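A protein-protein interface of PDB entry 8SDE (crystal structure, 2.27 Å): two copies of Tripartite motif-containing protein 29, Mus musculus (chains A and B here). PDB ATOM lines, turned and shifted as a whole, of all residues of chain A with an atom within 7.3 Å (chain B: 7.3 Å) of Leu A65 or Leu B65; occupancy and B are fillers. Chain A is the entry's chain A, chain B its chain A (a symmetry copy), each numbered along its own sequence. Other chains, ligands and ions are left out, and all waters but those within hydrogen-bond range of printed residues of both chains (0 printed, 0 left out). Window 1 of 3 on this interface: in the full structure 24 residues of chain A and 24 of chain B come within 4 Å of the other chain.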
ATOM      1  N   PHE A  58     -28.896  14.959  23.223  1.00  0.00           N
ATOM      2  CA  PHE A  58     -27.558  14.920  22.672  1.00  0.00           C
ATOM      3  C   PHE A  58     -27.360  16.134  21.777  1.00  0.00           C
ATOM      4  O   PHE A  58     -26.341  16.824  21.856  1.00  0.00           O
ATOM      5  CB  PHE A  58     -27.304  13.550  22.005  1.00  0.00           C
ATOM      6  CG  PHE A  58     -25.986  13.472  21.275  1.00  0.00           C
ATOM      7  CD1 PHE A  58     -24.801  13.255  21.960  1.00  0.00           C
ATOM      8  CD2 PHE A  58     -25.915  13.721  19.906  1.00  0.00           C
ATOM      9  CE1 PHE A  58     -23.578  13.288  21.291  1.00  0.00           C
ATOM     10  CE2 PHE A  58     -24.701  13.702  19.226  1.00  0.00           C
ATOM     11  CZ  PHE A  58     -23.536  13.461  19.923  1.00  0.00           C
ATOM     12  N   ARG A  59     -28.338  16.386  20.907  1.00  0.00           N
ATOM     13  CA  ARG A  59     -28.278  17.521  20.007  1.00  0.00           C
ATOM     14  C   ARG A  59     -28.270  18.838  20.760  1.00  0.00           C
ATOM     15  O   ARG A  59     -27.543  19.743  20.351  1.00  0.00           O
ATOM     16  CB  ARG A  59     -29.415  17.564  18.980  1.00  0.00           C
ATOM     17  CG  ARG A  59     -29.539  16.313  18.119  1.00  0.00           C
ATOM     18  CD  ARG A  59     -30.558  16.748  17.066  1.00  0.00           C
ATOM     19  NE  ARG A  59     -31.170  15.597  16.432  1.00  0.00           N
ATOM     20  CZ  ARG A  59     -30.530  14.742  15.638  1.00  0.00           C
ATOM     21  NH1 ARG A  59     -29.244  14.906  15.379  1.00  0.00           N
ATOM     22  NH2 ARG A  59     -31.179  13.717  15.112  1.00  0.00           N
ATOM     23  N   ASP A  60     -29.084  18.963  21.826  1.00  0.00           N
ATOM     24  CA  ASP A  60     -29.013  20.193  22.615  1.00  0.00           C
ATOM     25  C   ASP A  60     -27.641  20.294  23.290  1.00  0.00           C
ATOM     26  O   ASP A  60     -27.080  21.362  23.379  1.00  0.00           O
ATOM     27  CB  ASP A  60     -30.124  20.291  23.666  1.00  0.00           C
ATOM     28  CG  ASP A  60     -31.540  20.166  23.104  1.00  0.00           C
ATOM     29  OD1 ASP A  60     -31.735  20.533  21.929  1.00  0.00           O
ATOM     30  OD2 ASP A  60     -32.448  19.699  23.853  1.00  0.00           O
ATOM     31  N   LEU A  61     -27.108  19.189  23.832  1.00  0.00           N
ATOM     32  CA  LEU A  61     -25.798  19.263  24.460  1.00  0.00           C
ATOM     33  C   LEU A  61     -24.750  19.737  23.444  1.00  0.00           C
ATOM     34  O   LEU A  61     -24.012  20.692  23.706  1.00  0.00           O
ATOM     35  CB  LEU A  61     -25.488  17.861  25.014  1.00  0.00           C
ATOM     36  CG  LEU A  61     -24.126  17.638  25.667  1.00  0.00           C
ATOM     37  CD1 LEU A  61     -23.861  18.623  26.801  1.00  0.00           C
ATOM     38  CD2 LEU A  61     -24.041  16.218  26.184  1.00  0.00           C
ATOM     39  N   VAL A  62     -24.741  19.145  22.237  1.00  0.00           N
ATOM     40  CA  VAL A  62     -23.688  19.494  21.291  1.00  0.00           C
ATOM     41  C   VAL A  62     -23.793  20.971  20.936  1.00  0.00           C
ATOM     42  O   VAL A  62     -22.788  21.671  20.880  1.00  0.00           O
ATOM     43  CB  VAL A  62     -23.732  18.608  20.021  1.00  0.00           C
ATOM     44  CG1 VAL A  62     -22.775  19.129  18.957  1.00  0.00           C
ATOM     45  CG2 VAL A  62     -23.374  17.175  20.376  1.00  0.00           C
ATOM     46  N   ARG A  63     -25.018  21.430  20.641  1.00  0.00           N
ATOM     47  CA  ARG A  63     -25.252  22.840  20.366  1.00  0.00           C
ATOM     48  C   ARG A  63     -24.763  23.726  21.523  1.00  0.00           C
ATOM     49  O   ARG A  63     -24.175  24.778  21.308  1.00  0.00           O
ATOM     50  CB  ARG A  63     -26.748  23.033  20.103  1.00  0.00           C
ATOM     51  CG  ARG A  63     -27.215  24.482  20.037  1.00  0.00           C
ATOM     52  CD  ARG A  63     -28.538  24.595  19.297  1.00  0.00           C
ATOM     53  NE  ARG A  63     -29.719  24.579  20.151  1.00  0.00           N
ATOM     54  CZ  ARG A  63     -30.644  23.617  20.185  1.00  0.00           C
ATOM     55  NH1 ARG A  63     -30.548  22.557  19.397  1.00  0.00           N
ATOM     56  NH2 ARG A  63     -31.678  23.730  21.002  1.00  0.00           N
ATOM     57  N   GLU A  64     -25.033  23.346  22.778  1.00  0.00           N
ATOM     58  CA  GLU A  64     -24.571  24.199  23.861  1.00  0.00           C
ATOM     59  C   GLU A  64     -23.035  24.227  23.902  1.00  0.00           C
ATOM     60  O   GLU A  64     -22.457  25.260  24.248  1.00  0.00           O
ATOM     61  CB  GLU A  64     -25.161  23.756  25.206  1.00  0.00           C
ATOM     62  CG  GLU A  64     -24.788  24.657  26.383  1.00  0.00           C
ATOM     63  CD  GLU A  64     -24.806  26.183  26.194  1.00  0.00           C
ATOM     64  OE1 GLU A  64     -23.923  26.854  26.801  1.00  0.00           O
ATOM     65  OE2 GLU A  64     -25.691  26.722  25.442  1.00  0.00           O
ATOM     66  N   LEU A  65     -22.374  23.110  23.538  1.00  0.00           N
ATOM     67  CA  LEU A  65     -20.924  23.021  23.703  1.00  0.00           C
ATOM     68  C   LEU A  65     -20.252  23.771  22.568  1.00  0.00           C
ATOM     69  O   LEU A  65     -19.234  24.430  22.761  1.00  0.00           O
ATOM     70  CB  LEU A  65     -20.448  21.563  23.697  1.00  0.00           C
ATOM     71  CG  LEU A  65     -20.838  20.676  24.882  1.00  0.00           C
ATOM     72  CD1 LEU A  65     -20.637  19.211  24.474  1.00  0.00           C
ATOM     73  CD2 LEU A  65     -19.987  20.992  26.123  1.00  0.00           C
ATOM     74  N   GLU A  66     -20.834  23.647  21.376  1.00  0.00           N
ATOM     75  CA  GLU A  66     -20.378  24.406  20.237  1.00  0.00           C
ATOM     76  C   GLU A  66     -20.470  25.890  20.599  1.00  0.00           C
ATOM     77  O   GLU A  66     -19.518  26.633  20.407  1.00  0.00           O
ATOM     78  CB  GLU A  66     -21.213  24.006  19.015  1.00  0.00           C
ATOM     79  CG  GLU A  66     -20.940  24.837  17.776  1.00  0.00           C
ATOM     80  CD  GLU A  66     -19.691  24.474  16.982  1.00  0.00           C
ATOM     81  OE1 GLU A  66     -19.122  23.392  17.230  1.00  0.00           O
ATOM     82  OE2 GLU A  66     -19.289  25.273  16.101  1.00  0.00           O
ATOM     83  N   LYS A  67     -21.595  26.319  21.183  1.00  0.00           N
ATOM     84  CA  LYS A  67     -21.690  27.717  21.583  1.00  0.00           C
ATOM     85  C   LYS A  67     -20.626  28.083  22.625  1.00  0.00           C
ATOM     86  O   LYS A  67     -20.032  29.151  22.543  1.00  0.00           O
ATOM     87  CB  LYS A  67     -23.116  28.098  21.990  1.00  0.00           C
ATOM     88  CG  LYS A  67     -23.387  29.583  22.139  1.00  0.00           C
ATOM     89  CD  LYS A  67     -24.646  29.915  22.939  1.00  0.00           C
ATOM     90  CE  LYS A  67     -25.821  28.987  22.697  1.00  0.00           C
ATOM     91  NZ  LYS A  67     -26.692  28.892  23.899  1.00  0.00           N
ATOM     92  N   GLN A  68     -20.314  27.199  23.572  1.00  0.00           N
ATOM     93  CA  GLN A  68     -19.272  27.524  24.534  1.00  0.00           C
ATOM     94  C   GLN A  68     -17.903  27.612  23.842  1.00  0.00           C
ATOM     95  O   GLN A  68     -17.067  28.455  24.206  1.00  0.00           O
ATOM     96  CB  GLN A  68     -19.254  26.510  25.688  1.00  0.00           C
ATOM     97  CG  GLN A  68     -20.453  26.628  26.627  1.00  0.00           C
ATOM     98  CD  GLN A  68     -20.610  25.505  27.627  1.00  0.00           C
ATOM     99  OE1 GLN A  68     -19.701  24.698  27.864  1.00  0.00           O
ATOM    100  NE2 GLN A  68     -21.805  25.424  28.192  1.00  0.00           N
ATOM    101  N   LYS A  69     -17.691  26.770  22.816  1.00  0.00           N
ATOM    102  CA  LYS A  69     -16.400  26.743  22.148  1.00  0.00           C
ATOM    103  C   LYS A  69     -16.160  28.100  21.504  1.00  0.00           C
ATOM    104  O   LYS A  69     -15.035  28.618  21.535  1.00  0.00           O
ATOM    105  CB  LYS A  69     -16.269  25.549  21.178  1.00  0.00           C
ATOM    106  CG  LYS A  69     -15.042  25.607  20.271  1.00  0.00           C
ATOM    107  CD  LYS A  69     -15.019  24.586  19.174  1.00  0.00           C
ATOM    108  CE  LYS A  69     -16.089  24.835  18.139  1.00  0.00           C
ATOM    109  NZ  LYS A  69     -15.744  26.056  17.382  1.00  0.00           N
ATOM    110  N   GLU A  70     -17.256  28.676  20.974  1.00  0.00           N
ATOM    111  CA  GLU A  70     -17.271  29.933  20.230  1.00  0.00           C
ATOM    112  C   GLU A  70     -16.914  31.113  21.133  1.00  0.00           C
ATOM    113  O   GLU A  70     -16.187  32.025  20.728  1.00  0.00           O
ATOM    114  CB  GLU A  70     -18.657  30.139  19.633  1.00  0.00           C
ATOM    115  CG  GLU A  70     -18.735  30.019  18.121  1.00  0.00           C
ATOM    116  CD  GLU A  70     -18.080  28.821  17.458  1.00  0.00           C
ATOM    117  OE1 GLU A  70     -18.764  28.154  16.643  1.00  0.00           O
ATOM    118  OE2 GLU A  70     -16.882  28.582  17.722  1.00  0.00           O
ATOM    119  N   GLU A  71     -17.415  31.060  22.373  1.00  0.00           N
ATOM    120  CA  GLU A  71     -17.090  32.017  23.411  1.00  0.00           C
ATOM    121  C   GLU A  71     -15.602  31.923  23.760  1.00  0.00           C
ATOM    122  O   GLU A  71     -14.944  32.934  23.942  1.00  0.00           O
ATOM    123  CB  GLU A  71     -18.057  31.867  24.595  1.00  0.00           C
ATOM    124  CG  GLU A  71     -19.407  32.539  24.344  1.00  0.00           C
ATOM    125  CD  GLU A  71     -20.672  31.801  24.795  1.00  0.00           C
ATOM    126  OE1 GLU A  71     -20.749  31.402  25.984  1.00  0.00           O
ATOM    127  OE2 GLU A  71     -21.594  31.617  23.956  1.00  0.00           O
ATOM    128  N   PHE B  58     -12.536  19.917  21.024  1.00  0.00           N
ATOM    129  CA  PHE B  58     -13.969  19.942  20.829  1.00  0.00           C
ATOM    130  C   PHE B  58     -14.382  18.696  20.059  1.00  0.00           C
ATOM    131  O   PHE B  58     -15.343  18.015  20.419  1.00  0.00           O
ATOM    132  CB  PHE B  58     -14.390  21.288  20.197  1.00  0.00           C
ATOM    133  CG  PHE B  58     -15.850  21.344  19.821  1.00  0.00           C
ATOM    134  CD1 PHE B  58     -16.824  21.593  20.774  1.00  0.00           C
ATOM    135  CD2 PHE B  58     -16.264  21.044  18.524  1.00  0.00           C
ATOM    136  CE1 PHE B  58     -18.176  21.540  20.439  1.00  0.00           C
ATOM    137  CE2 PHE B  58     -17.611  21.044  18.173  1.00  0.00           C
ATOM    138  CZ  PHE B  58     -18.562  21.316  19.133  1.00  0.00           C
ATOM    139  N   ARG B  59     -13.653  18.407  18.981  1.00  0.00           N
ATOM    140  CA  ARG B  59     -13.933  17.240  18.168  1.00  0.00           C
ATOM    141  C   ARG B  59     -13.744  15.951  18.948  1.00  0.00           C
ATOM    142  O   ARG B  59     -14.547  15.035  18.771  1.00  0.00           O
ATOM    143  CB  ARG B  59     -13.093  17.152  16.890  1.00  0.00           C
ATOM    144  CG  ARG B  59     -13.197  18.369  15.979  1.00  0.00           C
ATOM    145  CD  ARG B  59     -12.475  17.890  14.720  1.00  0.00           C
ATOM    146  NE  ARG B  59     -12.049  19.013  13.908  1.00  0.00           N
ATOM    147  CZ  ARG B  59     -12.873  19.841  13.270  1.00  0.00           C
ATOM    148  NH1 ARG B  59     -14.182  19.673  13.351  1.00  0.00           N
ATOM    149  NH2 ARG B  59     -12.384  20.842  12.559  1.00  0.00           N
ATOM    150  N   ASP B  60     -12.687  15.863  19.777  1.00  0.00           N
ATOM    151  CA  ASP B  60     -12.550  14.664  20.605  1.00  0.00           C
ATOM    152  C   ASP B  60     -13.707  14.595  21.608  1.00  0.00           C
ATOM    153  O   ASP B  60     -14.222  13.534  21.876  1.00  0.00           O
ATOM    154  CB  ASP B  60     -11.209  14.600  21.343  1.00  0.00           C
ATOM    155  CG  ASP B  60      -9.982  14.697  20.437  1.00  0.00           C
ATOM    156  OD1 ASP B  60     -10.088  14.285  19.266  1.00  0.00           O
ATOM    157  OD2 ASP B  60      -8.916  15.188  20.914  1.00  0.00           O
ATOM    158  N   LEU B  61     -14.090  15.722  22.224  1.00  0.00           N
ATOM    159  CA  LEU B  61     -15.199  15.678  23.166  1.00  0.00           C
ATOM    160  C   LEU B  61     -16.467  15.172  22.467  1.00  0.00           C
ATOM    161  O   LEU B  61     -17.110  14.230  22.943  1.00  0.00           O
ATOM    162  CB  LEU B  61     -15.365  17.102  23.727  1.00  0.00           C
ATOM    163  CG  LEU B  61     -16.519  17.356  24.695  1.00  0.00           C
ATOM    164  CD1 LEU B  61     -16.484  16.415  25.895  1.00  0.00           C
ATOM    165  CD2 LEU B  61     -16.477  18.794  25.162  1.00  0.00           C
ATOM    166  N   VAL B  62     -16.784  15.717  21.280  1.00  0.00           N
ATOM    167  CA  VAL B  62     -18.040  15.338  20.644  1.00  0.00           C
ATOM    168  C   VAL B  62     -18.021  13.848  20.330  1.00  0.00           C
ATOM    169  O   VAL B  62     -19.005  13.152  20.557  1.00  0.00           O
ATOM    170  CB  VAL B  62     -18.323  16.176  19.373  1.00  0.00           C
ATOM    171  CG1 VAL B  62     -19.516  15.619  18.605  1.00  0.00           C
ATOM    172  CG2 VAL B  62     -18.587  17.623  19.752  1.00  0.00           C
ATOM    173  N   ARG B  63     -16.909  13.372  19.753  1.00  0.00           N
ATOM    174  CA  ARG B  63     -16.745  11.952  19.481  1.00  0.00           C
ATOM    175  C   ARG B  63     -16.921  11.113  20.757  1.00  0.00           C
ATOM    176  O   ARG B  63     -17.539  10.057  20.737  1.00  0.00           O
ATOM    177  CB  ARG B  63     -15.363  11.743  18.856  1.00  0.00           C
ATOM    178  CG  ARG B  63     -14.921  10.290  18.728  1.00  0.00           C
ATOM    179  CD  ARG B  63     -13.828  10.143  17.683  1.00  0.00           C
ATOM    180  NE  ARG B  63     -12.469  10.185  18.209  1.00  0.00           N
ATOM    181  CZ  ARG B  63     -11.570  11.143  17.972  1.00  0.00           C
ATOM    182  NH1 ARG B  63     -11.867  12.173  17.194  1.00  0.00           N
ATOM    183  NH2 ARG B  63     -10.363  11.056  18.505  1.00  0.00           N
ATOM    184  N   GLU B  64     -16.344  11.538  21.887  1.00  0.00           N
ATOM    185  CA  GLU B  64     -16.514  10.729  23.083  1.00  0.00           C
ATOM    186  C   GLU B  64     -17.989  10.710  23.512  1.00  0.00           C
ATOM    187  O   GLU B  64     -18.456   9.694  24.032  1.00  0.00           O
ATOM    188  CB  GLU B  64     -15.604  11.220  24.218  1.00  0.00           C
ATOM    189  CG  GLU B  64     -15.664  10.365  25.484  1.00  0.00           C
ATOM    190  CD  GLU B  64     -15.686   8.834  25.354  1.00  0.00           C
ATOM    191  OE1 GLU B  64     -16.384   8.190  26.190  1.00  0.00           O
ATOM    192  OE2 GLU B  64     -15.018   8.262  24.424  1.00  0.00           O
ATOM    193  N   LEU B  65     -18.726  11.816  23.285  1.00  0.00           N
ATOM    194  CA  LEU B  65     -20.088  11.918  23.808  1.00  0.00           C
ATOM    195  C   LEU B  65     -21.021  11.129  22.909  1.00  0.00           C
ATOM    196  O   LEU B  65     -21.953  10.483  23.378  1.00  0.00           O
ATOM    197  CB  LEU B  65     -20.557  13.377  23.868  1.00  0.00           C
ATOM    198  CG  LEU B  65     -19.884  14.306  24.881  1.00  0.00           C
ATOM    199  CD1 LEU B  65     -20.189  15.756  24.483  1.00  0.00           C
ATOM    200  CD2 LEU B  65     -20.392  14.041  26.309  1.00  0.00           C
ATOM    201  N   GLU B  66     -20.760  11.205  21.605  1.00  0.00           N
ATOM    202  CA  GLU B  66     -21.485  10.406  20.648  1.00  0.00           C
ATOM    203  C   GLU B  66     -21.297   8.937  21.030  1.00  0.00           C
ATOM    204  O   GLU B  66     -22.264   8.191  21.113  1.00  0.00           O
ATOM    205  CB  GLU B  66     -20.988  10.756  19.240  1.00  0.00           C
ATOM    206  CG  GLU B  66     -21.562   9.880  18.143  1.00  0.00           C
ATOM    207  CD  GLU B  66     -22.973  10.219  17.678  1.00  0.00           C
ATOM    208  OE1 GLU B  66     -23.466  11.312  18.020  1.00  0.00           O
ATOM    209  OE2 GLU B  66     -23.581   9.389  16.958  1.00  0.00           O
ATOM    210  N   LYS B  67     -20.059   8.524  21.327  1.00  0.00           N
ATOM    211  CA  LYS B  67     -19.860   7.141  21.742  1.00  0.00           C
ATOM    212  C   LYS B  67     -20.624   6.820  23.032  1.00  0.00           C
ATOM    213  O   LYS B  67     -21.214   5.753  23.144  1.00  0.00           O
ATOM    214  CB  LYS B  67     -18.376   6.770  21.789  1.00  0.00           C
ATOM    215  CG  LYS B  67     -18.068   5.290  21.921  1.00  0.00           C
ATOM    216  CD  LYS B  67     -16.646   4.982  22.389  1.00  0.00           C
ATOM    217  CE  LYS B  67     -15.576   5.894  21.822  1.00  0.00           C
ATOM    218  NZ  LYS B  67     -14.429   6.030  22.760  1.00  0.00           N
ATOM    219  N   GLN B  68     -20.691   7.741  23.993  1.00  0.00           N
ATOM    220  CA  GLN B  68     -21.454   7.458  25.199  1.00  0.00           C
ATOM    221  C   GLN B  68     -22.953   7.350  24.880  1.00  0.00           C
ATOM    222  O   GLN B  68     -23.666   6.525  25.475  1.00  0.00           O
ATOM    223  CB  GLN B  68     -21.184   8.515  26.281  1.00  0.00           C
ATOM    224  CG  GLN B  68     -19.786   8.426  26.890  1.00  0.00           C
ATOM    225  CD  GLN B  68     -19.387   9.585  27.775  1.00  0.00           C
ATOM    226  OE1 GLN B  68     -20.210  10.405  28.204  1.00  0.00           O
ATOM    227  NE2 GLN B  68     -18.089   9.682  28.016  1.00  0.00           N
ATOM    228  N   LYS B  69     -23.421   8.154  23.910  1.00  0.00           N
ATOM    229  CA  LYS B  69     -24.840   8.162  23.589  1.00  0.00           C
ATOM    230  C   LYS B  69     -25.228   6.783  23.078  1.00  0.00           C
ATOM    231  O   LYS B  69     -26.306   6.272  23.412  1.00  0.00           O
ATOM    232  CB  LYS B  69     -25.217   9.319  22.639  1.00  0.00           C
ATOM    233  CG  LYS B  69     -26.634   9.233  22.076  1.00  0.00           C
ATOM    234  CD  LYS B  69     -26.938  10.212  20.982  1.00  0.00           C
ATOM    235  CE  LYS B  69     -26.163   9.919  19.720  1.00  0.00           C
ATOM    236  NZ  LYS B  69     -26.683   8.672  19.122  1.00  0.00           N
ATOM    237  N   GLU B  70     -24.299   6.183  22.311  1.00  0.00           N
ATOM    238  CA  GLU B  70     -24.467   4.897  21.635  1.00  0.00           C
ATOM    239  C   GLU B  70     -24.578   3.754  22.642  1.00  0.00           C
ATOM    240  O   GLU B  70     -25.379   2.831  22.470  1.00  0.00           O
ATOM    241  CB  GLU B  70     -23.275   4.663  20.715  1.00  0.00           C
ATOM    242  CG  GLU B  70     -23.583   4.726  19.229  1.00  0.00           C
ATOM    243  CD  GLU B  70     -24.390   5.901  18.709  1.00  0.00           C
ATOM    244  OE1 GLU B  70     -23.937   6.533  17.723  1.00  0.00           O
ATOM    245  OE2 GLU B  70     -25.483   6.155  19.258  1.00  0.00           O
ATOM    246  N   GLU B  71     -23.780   3.852  23.713  1.00  0.00           N
ATOM    247  CA  GLU B  71     -23.827   2.937  24.835  1.00  0.00           C
ATOM    248  C   GLU B  71     -25.179   3.050  25.545  1.00  0.00           C
ATOM    249  O   GLU B  71     -25.765   2.050  25.926  1.00  0.00           O
ATOM    250  CB  GLU B  71     -22.592   3.126  25.729  1.00  0.00           C
ATOM    251  CG  GLU B  71     -21.347   2.438  25.171  1.00  0.00           C
ATOM    252  CD  GLU B  71     -20.013   3.187  25.259  1.00  0.00           C
ATOM    253  OE1 GLU B  71     -19.639   3.630  26.373  1.00  0.00           O
ATOM    254  OE2 GLU B  71     -19.334   3.335  24.208  1.00  0.00           O
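Phe A58 touches Leu B65, and with the chains exchanged Leu A65 touches Phe B58.
Phe A58 touches Glu B66, and with the chains exchanged Glu A66 touches Phe B58.
Phe A58 touches Lys B69, and with the chains exchanged Lys A69 touches Phe B58.
Leu B65 touches its own counterpart, Leu A65.
Of the 7 pairs that touch across the chains among the printed residues, 7 have their exchanged pair printed and touching as well.
Of chain B, only Phe B58 and Leu B65 come within 4 Å of Leu A65.
Of chain A, only Phe A58 and Leu A65 come within 4 Å of Leu B65.
Of the printed residues of chain B, Glu A66 touches Phe B58.
Of the printed residues of chain B, Phe A58 touches Leu B65, Glu B66 and Lys B69.
Arg B59 touches none of the printed residues of chain A.
Leu A61 touches none of the printed residues of chain B.
The nearest residue of chain B that does not touch Leu A65 is Leu B61 (4.2 Å).
The nearest residue of chain A that does not touch Leu B65 is Leu A61 (4.2 Å).
The nearest printed residue of chain A that does not touch Phe B58 is Val A62 (4.6 Å).
The side-chain carboxylate (OE2) of Glu A70 is in salt-bridge range of the side-chain amino group (NZ) of Lys A69 (2.8 Å).
OE2 of Glu B66 lies within salt-bridge range of NZ of Lys B69 (3.8 Å).
OE2 of Glu A66 lies within salt-bridge range of NZ of Lys A69.
OE2 of Glu B70 lies within salt-bridge range of NZ of Lys B69, 2.8 Å away.
Among the printed residues, pairs that only touch across the chains: Phe A58 with Leu B65, Phe A58 with Glu B66, Phe A58 with Lys B69, Leu A65 with Phe B58, Leu A65 with Leu B65, Glu A66 with Phe B58 and Lys A69 with Phe B58.
Hydrophobic or aromatic side chains of chain A that line the printed part of chain B: Phe A58 and Leu A65.
Hydrophobic or aromatic side chains of chain B within 4 Å of the printed part of chain A: Phe B58 and Leu B65.
Among the printed residues, no Asp or Glu carboxylate lies within 4 Å of a Lys or Arg side-chain nitrogen of the other chain.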
